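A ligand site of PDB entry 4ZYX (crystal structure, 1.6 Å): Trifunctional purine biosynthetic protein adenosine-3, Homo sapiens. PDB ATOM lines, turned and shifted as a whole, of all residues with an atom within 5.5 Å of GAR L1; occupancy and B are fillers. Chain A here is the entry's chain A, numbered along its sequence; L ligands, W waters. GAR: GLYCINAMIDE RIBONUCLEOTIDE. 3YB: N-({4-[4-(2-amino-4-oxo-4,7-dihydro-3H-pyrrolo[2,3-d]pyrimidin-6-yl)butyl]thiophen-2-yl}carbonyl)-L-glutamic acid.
The backbone carbonyl oxygen (O) of Lys 171 sits close to a ring nitrogen (ND1) of His 175, at 3.3 Å.
A ring nitrogen (NE2) of His 175 is in hydrogen-bond range of the side-chain hydroxyl of Ser 13 (2.8 Å).
The side-chain carboxylate (OE1) of Glu 174 is in hydrogen-bond range of the side-chain amide nitrogen (ND2) of Asn 14 (2.8 Å).
Thr 11 touches GAR L1.
Gly 88 touches GAR L1.
SD of Met 90 touches C23 of GAR L1, at 3.8 Å.
Asn 107 touches GAR L1 (OD1 to N24, 3.9 Å).
Pro 110 touches GAR L1 (CD to O8, 3.3 Å).
Within 4 Å of GAR L1: Thr 11, Gly 12, Ser 13, Asn 14, Gly 88, Met 90, Asn 107, Ile 108, Pro 110, Lys 171 and Glu 174.
Water W7 bridges an oxygen (O17) of GAR L1 (2.7 Å) and the backbone NH (N) of Thr 11 (3.0 Å).
Water W8 lies within hydrogen-bond range of an oxygen (O6) of GAR L1 and a ring nitrogen (NE2) of His 122.
Water W5 lies within hydrogen-bond range of an oxygen (O18) of GAR L1 (2.7 Å), the backbone NH of Leu 15 (2.9 Å), the backbone carbonyl oxygen of Ala 87 (2.9 Å) and the backbone NH of Asn 14 (3.3 Å).
Water W6 lies within hydrogen-bond range of the side-chain carboxylate (OD1) of Asp 145 (2.6 Å), a ring nitrogen (ND1) of His 109 (2.8 Å), a nitrogen (N24) of GAR L1 (2.8 Å) and the side-chain amide nitrogen (ND2) of Asn 107 (3.0 Å).
Water W9 lies within hydrogen-bond range of O of Ala 87 (2.9 Å), O17 of GAR L1 (2.9 Å), N of Gly 10 (3.1 Å) and O of Gly 88 (3.5 Å).
Water W3 lies within hydrogen-bond range of O of Ile 108 (2.7 Å), N of Gly 88 (2.9 Å) and N19 of GAR L1 (2.9 Å).
The side-chain hydroxyl of Ser 13 sits at hydrogen-bond distance from an oxygen (O16) of GAR L1 (2.6 Å).
The side-chain carboxylate (OE1) of Glu 174 sits at hydrogen-bond distance from an oxygen (O8) of GAR L1, at 2.7 Å.
N of Asn 14 is in hydrogen-bond range of O18 of GAR L1, at 3.0 Å.
An oxygen (O16) of GAR L1 is in salt-bridge range of the side-chain amino group (NZ) of Lys 171 (3.0 Å).
The backbone carbonyl oxygen of Met 90 sits at hydrogen-bond distance from a nitrogen (N19) of 3YB L2 (3.1 Å).
The side-chain amide nitrogen of Asn 14 sits at hydrogen-bond distance from an oxygen (O18) of GAR L1, at 3.1 Å.
The backbone carbonyl oxygen (O) of Ile 108 lies within hydrogen-bond range of a nitrogen (N24) of GAR L1 (3.1 Å).
An oxygen (O16) of GAR L1 is in hydrogen-bond range of the backbone NH (N) of Ser 13, at 2.9 Å.
N of Gly 12 is in hydrogen-bond range of O17 of GAR L1, 2.9 Å away.
N of Asp 145 sits at hydrogen-bond distance from O10 of 3YB L2, 3.1 Å away.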
ATOM      1  N   GLY A  10     -22.258 -11.538 -32.525  1.00  0.00           N
ATOM      2  CA  GLY A  10     -23.230 -12.610 -32.566  1.00  0.00           C
ATOM      3  C   GLY A  10     -24.606 -12.378 -31.964  1.00  0.00           C
ATOM      4  O   GLY A  10     -25.267 -11.391 -32.274  1.00  0.00           O
ATOM      5  N   THR A  11     -25.032 -13.321 -31.113  1.00  0.00           N
ATOM      6  CA  THR A  11     -26.402 -13.384 -30.617  1.00  0.00           C
ATOM      7  C   THR A  11     -26.842 -12.133 -29.854  1.00  0.00           C
ATOM      8  O   THR A  11     -27.956 -11.630 -30.031  1.00  0.00           O
ATOM      9  CB  THR A  11     -26.583 -14.600 -29.693  1.00  0.00           C
ATOM     10  OG1 THR A  11     -26.227 -15.799 -30.407  1.00  0.00           O
ATOM     11  CG2 THR A  11     -28.018 -14.710 -29.198  1.00  0.00           C
ATOM     12  N   GLY A  12     -25.971 -11.654 -28.977  1.00  0.00           N
ATOM     13  CA  GLY A  12     -26.235 -10.415 -28.270  1.00  0.00           C
ATOM     14  C   GLY A  12     -26.998 -10.523 -26.969  1.00  0.00           C
ATOM     15  O   GLY A  12     -27.641  -9.540 -26.558  1.00  0.00           O
ATOM     16  N   SER A  13     -26.939 -11.667 -26.297  1.00  0.00           N
ATOM     17  CA  SER A  13     -27.605 -11.761 -24.993  1.00  0.00           C
ATOM     18  C   SER A  13     -26.937 -10.826 -23.990  1.00  0.00           C
ATOM     19  O   SER A  13     -27.636 -10.208 -23.181  1.00  0.00           O
ATOM     20  CB  SER A  13     -27.639 -13.207 -24.450  1.00  0.00           C
ATOM     21  OG  SER A  13     -26.363 -13.628 -24.020  1.00  0.00           O
ATOM     22  N   ASN A  14     -25.608 -10.702 -24.027  1.00  0.00           N
ATOM     23  CA  ASN A  14     -24.973  -9.745 -23.120  1.00  0.00           C
ATOM     24  C   ASN A  14     -25.373  -8.312 -23.448  1.00  0.00           C
ATOM     25  O   ASN A  14     -25.634  -7.516 -22.543  1.00  0.00           O
ATOM     26  CB  ASN A  14     -23.452  -9.897 -23.132  1.00  0.00           C
ATOM     27  CG  ASN A  14     -22.968 -10.960 -22.142  1.00  0.00           C
ATOM     28  OD1 ASN A  14     -23.008 -10.745 -20.933  1.00  0.00           O
ATOM     29  ND2 ASN A  14     -22.518 -12.104 -22.653  1.00  0.00           N
ATOM     30  N   LEU A  15     -25.422  -7.987 -24.741  1.00  0.00           N
ATOM     31  CA  LEU A  15     -25.916  -6.677 -25.168  1.00  0.00           C
ATOM     32  C   LEU A  15     -27.309  -6.407 -24.599  1.00  0.00           C
ATOM     33  O   LEU A  15     -27.562  -5.319 -24.065  1.00  0.00           O
ATOM     34  CB  LEU A  15     -25.963  -6.579 -26.695  1.00  0.00           C
ATOM     35  CG  LEU A  15     -26.777  -5.403 -27.222  1.00  0.00           C
ATOM     36  CD1 LEU A  15     -26.141  -4.075 -26.843  1.00  0.00           C
ATOM     37  CD2 LEU A  15     -26.924  -5.524 -28.730  1.00  0.00           C
ATOM     38  N   ALA A  87     -18.910  -7.333 -26.043  1.00  0.00           N
ATOM     39  CA  ALA A  87     -19.964  -8.232 -25.569  1.00  0.00           C
ATOM     40  C   ALA A  87     -20.188  -9.318 -26.612  1.00  0.00           C
ATOM     41  O   ALA A  87     -21.042  -9.187 -27.485  1.00  0.00           O
ATOM     42  CB  ALA A  87     -21.242  -7.449 -25.304  1.00  0.00           C
ATOM     43  N   GLY A  88     -19.395 -10.372 -26.539  1.00  0.00           N
ATOM     44  CA  GLY A  88     -19.415 -11.394 -27.565  1.00  0.00           C
ATOM     45  C   GLY A  88     -18.688 -10.990 -28.831  1.00  0.00           C
ATOM     46  O   GLY A  88     -18.793 -11.658 -29.851  1.00  0.00           O
ATOM     47  N   PHE A  89     -17.941  -9.877 -28.779  1.00  0.00           N
ATOM     48  CA  PHE A  89     -17.076  -9.435 -29.863  1.00  0.00           C
ATOM     49  C   PHE A  89     -15.849 -10.335 -29.907  1.00  0.00           C
ATOM     50  O   PHE A  89     -15.142 -10.471 -28.928  1.00  0.00           O
ATOM     51  CB  PHE A  89     -16.669  -7.977 -29.627  1.00  0.00           C
ATOM     52  CG  PHE A  89     -15.831  -7.382 -30.718  1.00  0.00           C
ATOM     53  CD1 PHE A  89     -16.413  -6.960 -31.897  1.00  0.00           C
ATOM     54  CD2 PHE A  89     -14.464  -7.223 -30.543  1.00  0.00           C
ATOM     55  CE1 PHE A  89     -15.640  -6.388 -32.899  1.00  0.00           C
ATOM     56  CE2 PHE A  89     -13.675  -6.646 -31.539  1.00  0.00           C
ATOM     57  CZ  PHE A  89     -14.264  -6.237 -32.708  1.00  0.00           C
ATOM     58  N   MET A  90     -15.587 -10.972 -31.045  1.00  0.00           N
ATOM     59  CA  MET A  90     -14.583 -12.025 -31.029  1.00  0.00           C
ATOM     60  C   MET A  90     -13.252 -11.683 -31.723  1.00  0.00           C
ATOM     61  O   MET A  90     -12.452 -12.584 -31.966  1.00  0.00           O
ATOM     62  CB  MET A  90     -15.170 -13.309 -31.640  1.00  0.00           C
ATOM     63  CG  MET A  90     -16.277 -13.965 -30.807  1.00  0.00           C
ATOM     64  SD  MET A  90     -15.846 -14.274 -29.066  1.00  0.00           S
ATOM     65  CE  MET A  90     -14.662 -15.611 -29.274  1.00  0.00           C
ATOM     66  N   ASN A 107     -14.337  -6.110 -21.205  1.00  0.00           N
ATOM     67  CA  ASN A 107     -14.663  -7.348 -21.916  1.00  0.00           C
ATOM     68  C   ASN A 107     -15.289  -8.348 -20.980  1.00  0.00           C
ATOM     69  O   ASN A 107     -14.933  -8.384 -19.800  1.00  0.00           O
ATOM     70  CB  ASN A 107     -13.410  -7.949 -22.552  1.00  0.00           C
ATOM     71  CG  ASN A 107     -13.690  -9.238 -23.316  1.00  0.00           C
ATOM     72  OD1 ASN A 107     -14.500  -9.253 -24.251  1.00  0.00           O
ATOM     73  ND2 ASN A 107     -13.011 -10.315 -22.925  1.00  0.00           N
ATOM     74  N   ILE A 108     -16.218  -9.149 -21.486  1.00  0.00           N
ATOM     75  CA  ILE A 108     -16.750 -10.282 -20.724  1.00  0.00           C
ATOM     76  C   ILE A 108     -16.157 -11.577 -21.269  1.00  0.00           C
ATOM     77  O   ILE A 108     -16.086 -11.799 -22.486  1.00  0.00           O
ATOM     78  CB  ILE A 108     -18.308 -10.351 -20.743  1.00  0.00           C
ATOM     79  CG1 ILE A 108     -18.848 -11.500 -19.896  1.00  0.00           C
ATOM     80  CG2 ILE A 108     -18.855 -10.463 -22.157  1.00  0.00           C
ATOM     81  CD1 ILE A 108     -18.883 -11.195 -18.441  1.00  0.00           C
ATOM     82  N   HIS A 109     -15.691 -12.421 -20.357  1.00  0.00           N
ATOM     83  CA  HIS A 109     -15.031 -13.666 -20.724  1.00  0.00           C
ATOM     84  C   HIS A 109     -15.626 -14.798 -19.912  1.00  0.00           C
ATOM     85  O   HIS A 109     -15.734 -14.683 -18.704  1.00  0.00           O
ATOM     86  CB  HIS A 109     -13.526 -13.558 -20.490  1.00  0.00           C
ATOM     87  CG  HIS A 109     -12.780 -14.805 -20.832  1.00  0.00           C
ATOM     88  ND1 HIS A 109     -12.399 -15.103 -22.126  1.00  0.00           N
ATOM     89  CD2 HIS A 109     -12.361 -15.837 -20.066  1.00  0.00           C
ATOM     90  CE1 HIS A 109     -11.774 -16.264 -22.140  1.00  0.00           C
ATOM     91  NE2 HIS A 109     -11.736 -16.732 -20.901  1.00  0.00           N
ATOM     92  N   PRO A 110     -16.009 -15.914 -20.578  1.00  0.00           N
ATOM     93  CA  PRO A 110     -16.739 -16.976 -19.880  1.00  0.00           C
ATOM     94  C   PRO A 110     -15.851 -18.009 -19.194  1.00  0.00           C
ATOM     95  O   PRO A 110     -16.045 -19.219 -19.347  1.00  0.00           O
ATOM     96  CB  PRO A 110     -17.531 -17.638 -21.024  1.00  0.00           C
ATOM     97  CG  PRO A 110     -16.613 -17.513 -22.190  1.00  0.00           C
ATOM     98  CD  PRO A 110     -15.921 -16.157 -22.031  1.00  0.00           C
ATOM     99  N   GLY A 118      -8.716 -17.376 -23.982  1.00  0.00           N
ATOM    100  CA  GLY A 118      -8.904 -17.712 -25.376  1.00  0.00           C
ATOM    101  C   GLY A 118     -10.346 -17.765 -25.820  1.00  0.00           C
ATOM    102  O   GLY A 118     -11.255 -17.394 -25.071  1.00  0.00           O
ATOM    103  N   SER A 119     -10.573 -18.266 -27.025  1.00  0.00           N
ATOM    104  CA  SER A 119     -11.886 -18.175 -27.644  1.00  0.00           C
ATOM    105  C   SER A 119     -12.788 -19.364 -27.382  1.00  0.00           C
ATOM    106  O   SER A 119     -13.967 -19.333 -27.755  1.00  0.00           O
ATOM    107  CB  SER A 119     -11.737 -17.976 -29.154  1.00  0.00           C
ATOM    108  OG  SER A 119     -11.154 -19.142 -29.714  1.00  0.00           O
ATOM    109  N   HIS A 122     -15.169 -22.676 -22.631  1.00  0.00           N
ATOM    110  CA  HIS A 122     -15.979 -23.776 -22.135  1.00  0.00           C
ATOM    111  C   HIS A 122     -15.394 -25.125 -22.551  1.00  0.00           C
ATOM    112  O   HIS A 122     -15.393 -26.065 -21.753  1.00  0.00           O
ATOM    113  CB  HIS A 122     -17.433 -23.679 -22.620  1.00  0.00           C
ATOM    114  CG  HIS A 122     -18.145 -22.463 -22.124  1.00  0.00           C
ATOM    115  ND1 HIS A 122     -18.240 -22.156 -20.785  1.00  0.00           N
ATOM    116  CD2 HIS A 122     -18.803 -21.482 -22.792  1.00  0.00           C
ATOM    117  CE1 HIS A 122     -18.929 -21.032 -20.641  1.00  0.00           C
ATOM    118  NE2 HIS A 122     -19.265 -20.600 -21.842  1.00  0.00           N
ATOM    119  N   ASP A 145      -7.096 -11.288 -22.660  1.00  0.00           N
ATOM    120  CA  ASP A 145      -7.677 -11.862 -21.440  1.00  0.00           C
ATOM    121  C   ASP A 145      -6.751 -11.758 -20.233  1.00  0.00           C
ATOM    122  O   ASP A 145      -6.850 -12.554 -19.290  1.00  0.00           O
ATOM    123  CB  ASP A 145      -8.065 -13.335 -21.682  1.00  0.00           C
ATOM    124  CG  ASP A 145      -9.135 -13.488 -22.755  1.00  0.00           C
ATOM    125  OD1 ASP A 145      -9.867 -12.503 -23.026  1.00  0.00           O
ATOM    126  OD2 ASP A 145      -9.260 -14.581 -23.329  1.00  0.00           O
ATOM    127  N   LYS A 171     -23.954 -17.886 -18.943  1.00  0.00           N
ATOM    128  CA  LYS A 171     -24.511 -16.642 -19.443  1.00  0.00           C
ATOM    129  C   LYS A 171     -25.436 -15.961 -18.435  1.00  0.00           C
ATOM    130  O   LYS A 171     -25.529 -14.744 -18.406  1.00  0.00           O
ATOM    131  CB  LYS A 171     -25.245 -16.875 -20.763  1.00  0.00           C
ATOM    132  CG  LYS A 171     -24.298 -16.892 -21.957  1.00  0.00           C
ATOM    133  CD  LYS A 171     -25.050 -17.002 -23.265  1.00  0.00           C
ATOM    134  CE  LYS A 171     -24.099 -16.988 -24.457  1.00  0.00           C
ATOM    135  NZ  LYS A 171     -24.843 -16.819 -25.752  1.00  0.00           N
ATOM    136  N   GLU A 174     -23.110 -13.972 -16.541  1.00  0.00           N
ATOM    137  CA  GLU A 174     -22.556 -12.893 -17.356  1.00  0.00           C
ATOM    138  C   GLU A 174     -23.511 -11.710 -17.346  1.00  0.00           C
ATOM    139  O   GLU A 174     -23.093 -10.556 -17.224  1.00  0.00           O
ATOM    140  CB  GLU A 174     -22.316 -13.361 -18.799  1.00  0.00           C
ATOM    141  CG  GLU A 174     -21.280 -14.458 -18.937  1.00  0.00           C
ATOM    142  CD  GLU A 174     -21.105 -14.897 -20.376  1.00  0.00           C
ATOM    143  OE1 GLU A 174     -21.023 -14.000 -21.245  1.00  0.00           O
ATOM    144  OE2 GLU A 174     -21.033 -16.129 -20.629  1.00  0.00           O
ATOM    145  N   HIS A 175     -24.799 -12.021 -17.468  1.00  0.00           N
ATOM    146  CA  HIS A 175     -25.820 -10.985 -17.547  1.00  0.00           C
ATOM    147  C   HIS A 175     -26.012 -10.231 -16.236  1.00  0.00           C
ATOM    148  O   HIS A 175     -26.695  -9.215 -16.202  1.00  0.00           O
ATOM    149  CB  HIS A 175     -27.147 -11.594 -17.979  1.00  0.00           C
ATOM    150  CG  HIS A 175     -27.078 -12.259 -19.311  1.00  0.00           C
ATOM    151  ND1 HIS A 175     -28.041 -13.152 -19.745  1.00  0.00           N
ATOM    152  CD2 HIS A 175     -26.164 -12.172 -20.306  1.00  0.00           C
ATOM    153  CE1 HIS A 175     -27.713 -13.586 -20.954  1.00  0.00           C
ATOM    154  NE2 HIS A 175     -26.582 -13.014 -21.314  1.00  0.00           N
HETATM  155  C1  GAR L   1     -20.549 -14.877 -24.170  1.00  0.00           C
HETATM  156  O6  GAR L   1     -20.682 -16.101 -23.455  1.00  0.00           O
HETATM  157  C2  GAR L   1     -19.181 -14.288 -23.936  1.00  0.00           C
HETATM  158  O8  GAR L   1     -18.698 -14.429 -22.593  1.00  0.00           O
HETATM  159  C3  GAR L   1     -18.324 -15.077 -24.924  1.00  0.00           C
HETATM  160  O4  GAR L   1     -19.163 -15.127 -26.076  1.00  0.00           O
HETATM  161  C5  GAR L   1     -20.535 -15.196 -25.658  1.00  0.00           C
HETATM  162  C10 GAR L   1     -21.340 -14.156 -26.401  1.00  0.00           C
HETATM  163  O12 GAR L   1     -22.725 -14.357 -26.158  1.00  0.00           O
HETATM  164  N19 GAR L   1     -17.049 -14.432 -25.177  1.00  0.00           N
HETATM  165  C21 GAR L   1     -15.950 -15.165 -25.338  1.00  0.00           C
HETATM  166  O22 GAR L   1     -15.947 -16.382 -25.418  1.00  0.00           O
HETATM  167  C23 GAR L   1     -14.642 -14.413 -25.454  1.00  0.00           C
HETATM  168  N24 GAR L   1     -14.781 -13.035 -25.061  1.00  0.00           N
HETATM  169  P15 GAR L   1     -23.785 -13.197 -26.529  1.00  0.00           P
HETATM  170  O16 GAR L   1     -25.119 -13.885 -26.290  1.00  0.00           O
HETATM  171  O17 GAR L   1     -23.492 -12.842 -27.977  1.00  0.00           O
HETATM  172  O18 GAR L   1     -23.451 -12.082 -25.596  1.00  0.00           O
HETATM  173  N1  3YB L   2      -8.011  -7.737 -27.681  1.00  0.00           N
HETATM  174  C2  3YB L   2      -6.991  -7.505 -26.853  1.00  0.00           C
HETATM  175  N3  3YB L   2      -7.075  -7.828 -25.546  1.00  0.00           N
HETATM  176  C4  3YB L   2      -8.180  -8.407 -25.028  1.00  0.00           C
HETATM  177  N5  3YB L   2     -10.256  -8.610 -27.866  1.00  0.00           N
HETATM  178  C6  3YB L   2     -11.136  -9.185 -27.019  1.00  0.00           C
HETATM  179  C7  3YB L   2     -10.561  -9.205 -25.753  1.00  0.00           C
HETATM  180  C8  3YB L   2      -9.272  -8.655 -25.873  1.00  0.00           C
HETATM  181  C9  3YB L   2      -9.138  -8.301 -27.218  1.00  0.00           C
HETATM  182  O10 3YB L   2      -8.178  -8.678 -23.818  1.00  0.00           O
HETATM  183  N11 3YB L   2      -5.786  -6.904 -27.329  1.00  0.00           N
HETATM  184  C12 3YB L   2     -10.574 -14.046 -29.705  1.00  0.00           C
HETATM  185  C13 3YB L   2      -9.509 -14.704 -30.238  1.00  0.00           C
HETATM  186  S14 3YB L   2      -8.647 -15.292 -28.887  1.00  0.00           S
HETATM  187  C15 3YB L   2      -9.657 -14.689 -27.644  1.00  0.00           C
HETATM  188  C16 3YB L   2     -10.668 -14.043 -28.285  1.00  0.00           C
HETATM  189  C17 3YB L   2      -9.169 -14.842 -31.640  1.00  0.00           C
HETATM  190  O18 3YB L   2      -8.261 -15.604 -31.936  1.00  0.00           O
HETATM  191  N19 3YB L   2      -9.875 -14.094 -32.642  1.00  0.00           N
HETATM  192  C20 3YB L   2      -9.572 -14.197 -33.955  1.00  0.00           C
HETATM  193  C21 3YB L   2     -10.746 -14.343 -34.739  1.00  0.00           C
HETATM  194  C22 3YB L   2     -11.809 -15.085 -34.013  1.00  0.00           C
HETATM  195  C23 3YB L   2     -13.071 -15.058 -34.808  1.00  0.00           C
HETATM  196  O24 3YB L   2     -13.299 -14.085 -35.599  1.00  0.00           O
HETATM  197  O25 3YB L   2     -13.902 -15.994 -34.695  1.00  0.00           O
HETATM  198  C26 3YB L   2      -8.908 -13.035 -34.411  1.00  0.00           C
HETATM  199  O27 3YB L   2      -8.117 -13.125 -35.390  1.00  0.00           O
HETATM  200  O28 3YB L   2      -9.101 -11.909 -33.880  1.00  0.00           O
HETATM  201  C29 3YB L   2     -12.502  -9.645 -27.401  1.00  0.00           C
HETATM  202  C30 3YB L   2     -12.634 -11.113 -27.092  1.00  0.00           C
HETATM  203  C31 3YB L   2     -11.652 -11.889 -27.879  1.00  0.00           C
HETATM  204  C32 3YB L   2     -11.776 -13.343 -27.579  1.00  0.00           C
HETATM  205  O   HOH W   1     -21.217 -18.592 -21.326  1.00  0.00           O
HETATM  206  O   HOH W   2     -17.707 -18.436 -25.786  1.00  0.00           O
HETATM  207  O   HOH W   3     -17.345 -11.520 -24.882  1.00  0.00           O
HETATM  208  O   HOH W   4     -13.969 -18.243 -24.646  1.00  0.00           O
HETATM  209  O   HOH W   5     -23.790  -9.540 -26.531  1.00  0.00           O
HETATM  210  O   HOH W   6     -12.233 -13.053 -23.972  1.00  0.00           O
HETATM  211  O   HOH W   7     -22.813 -14.715 -29.743  1.00  0.00           O
HETATM  212  O   HOH W   8     -20.234 -18.658 -24.296  1.00  0.00           O
HETATM  213  O   HOH W   9     -22.144 -10.817 -29.561  1.00  0.00           O
HETATM  214  O   HOH W  10     -19.174 -16.216 -28.708  1.00  0.00           O
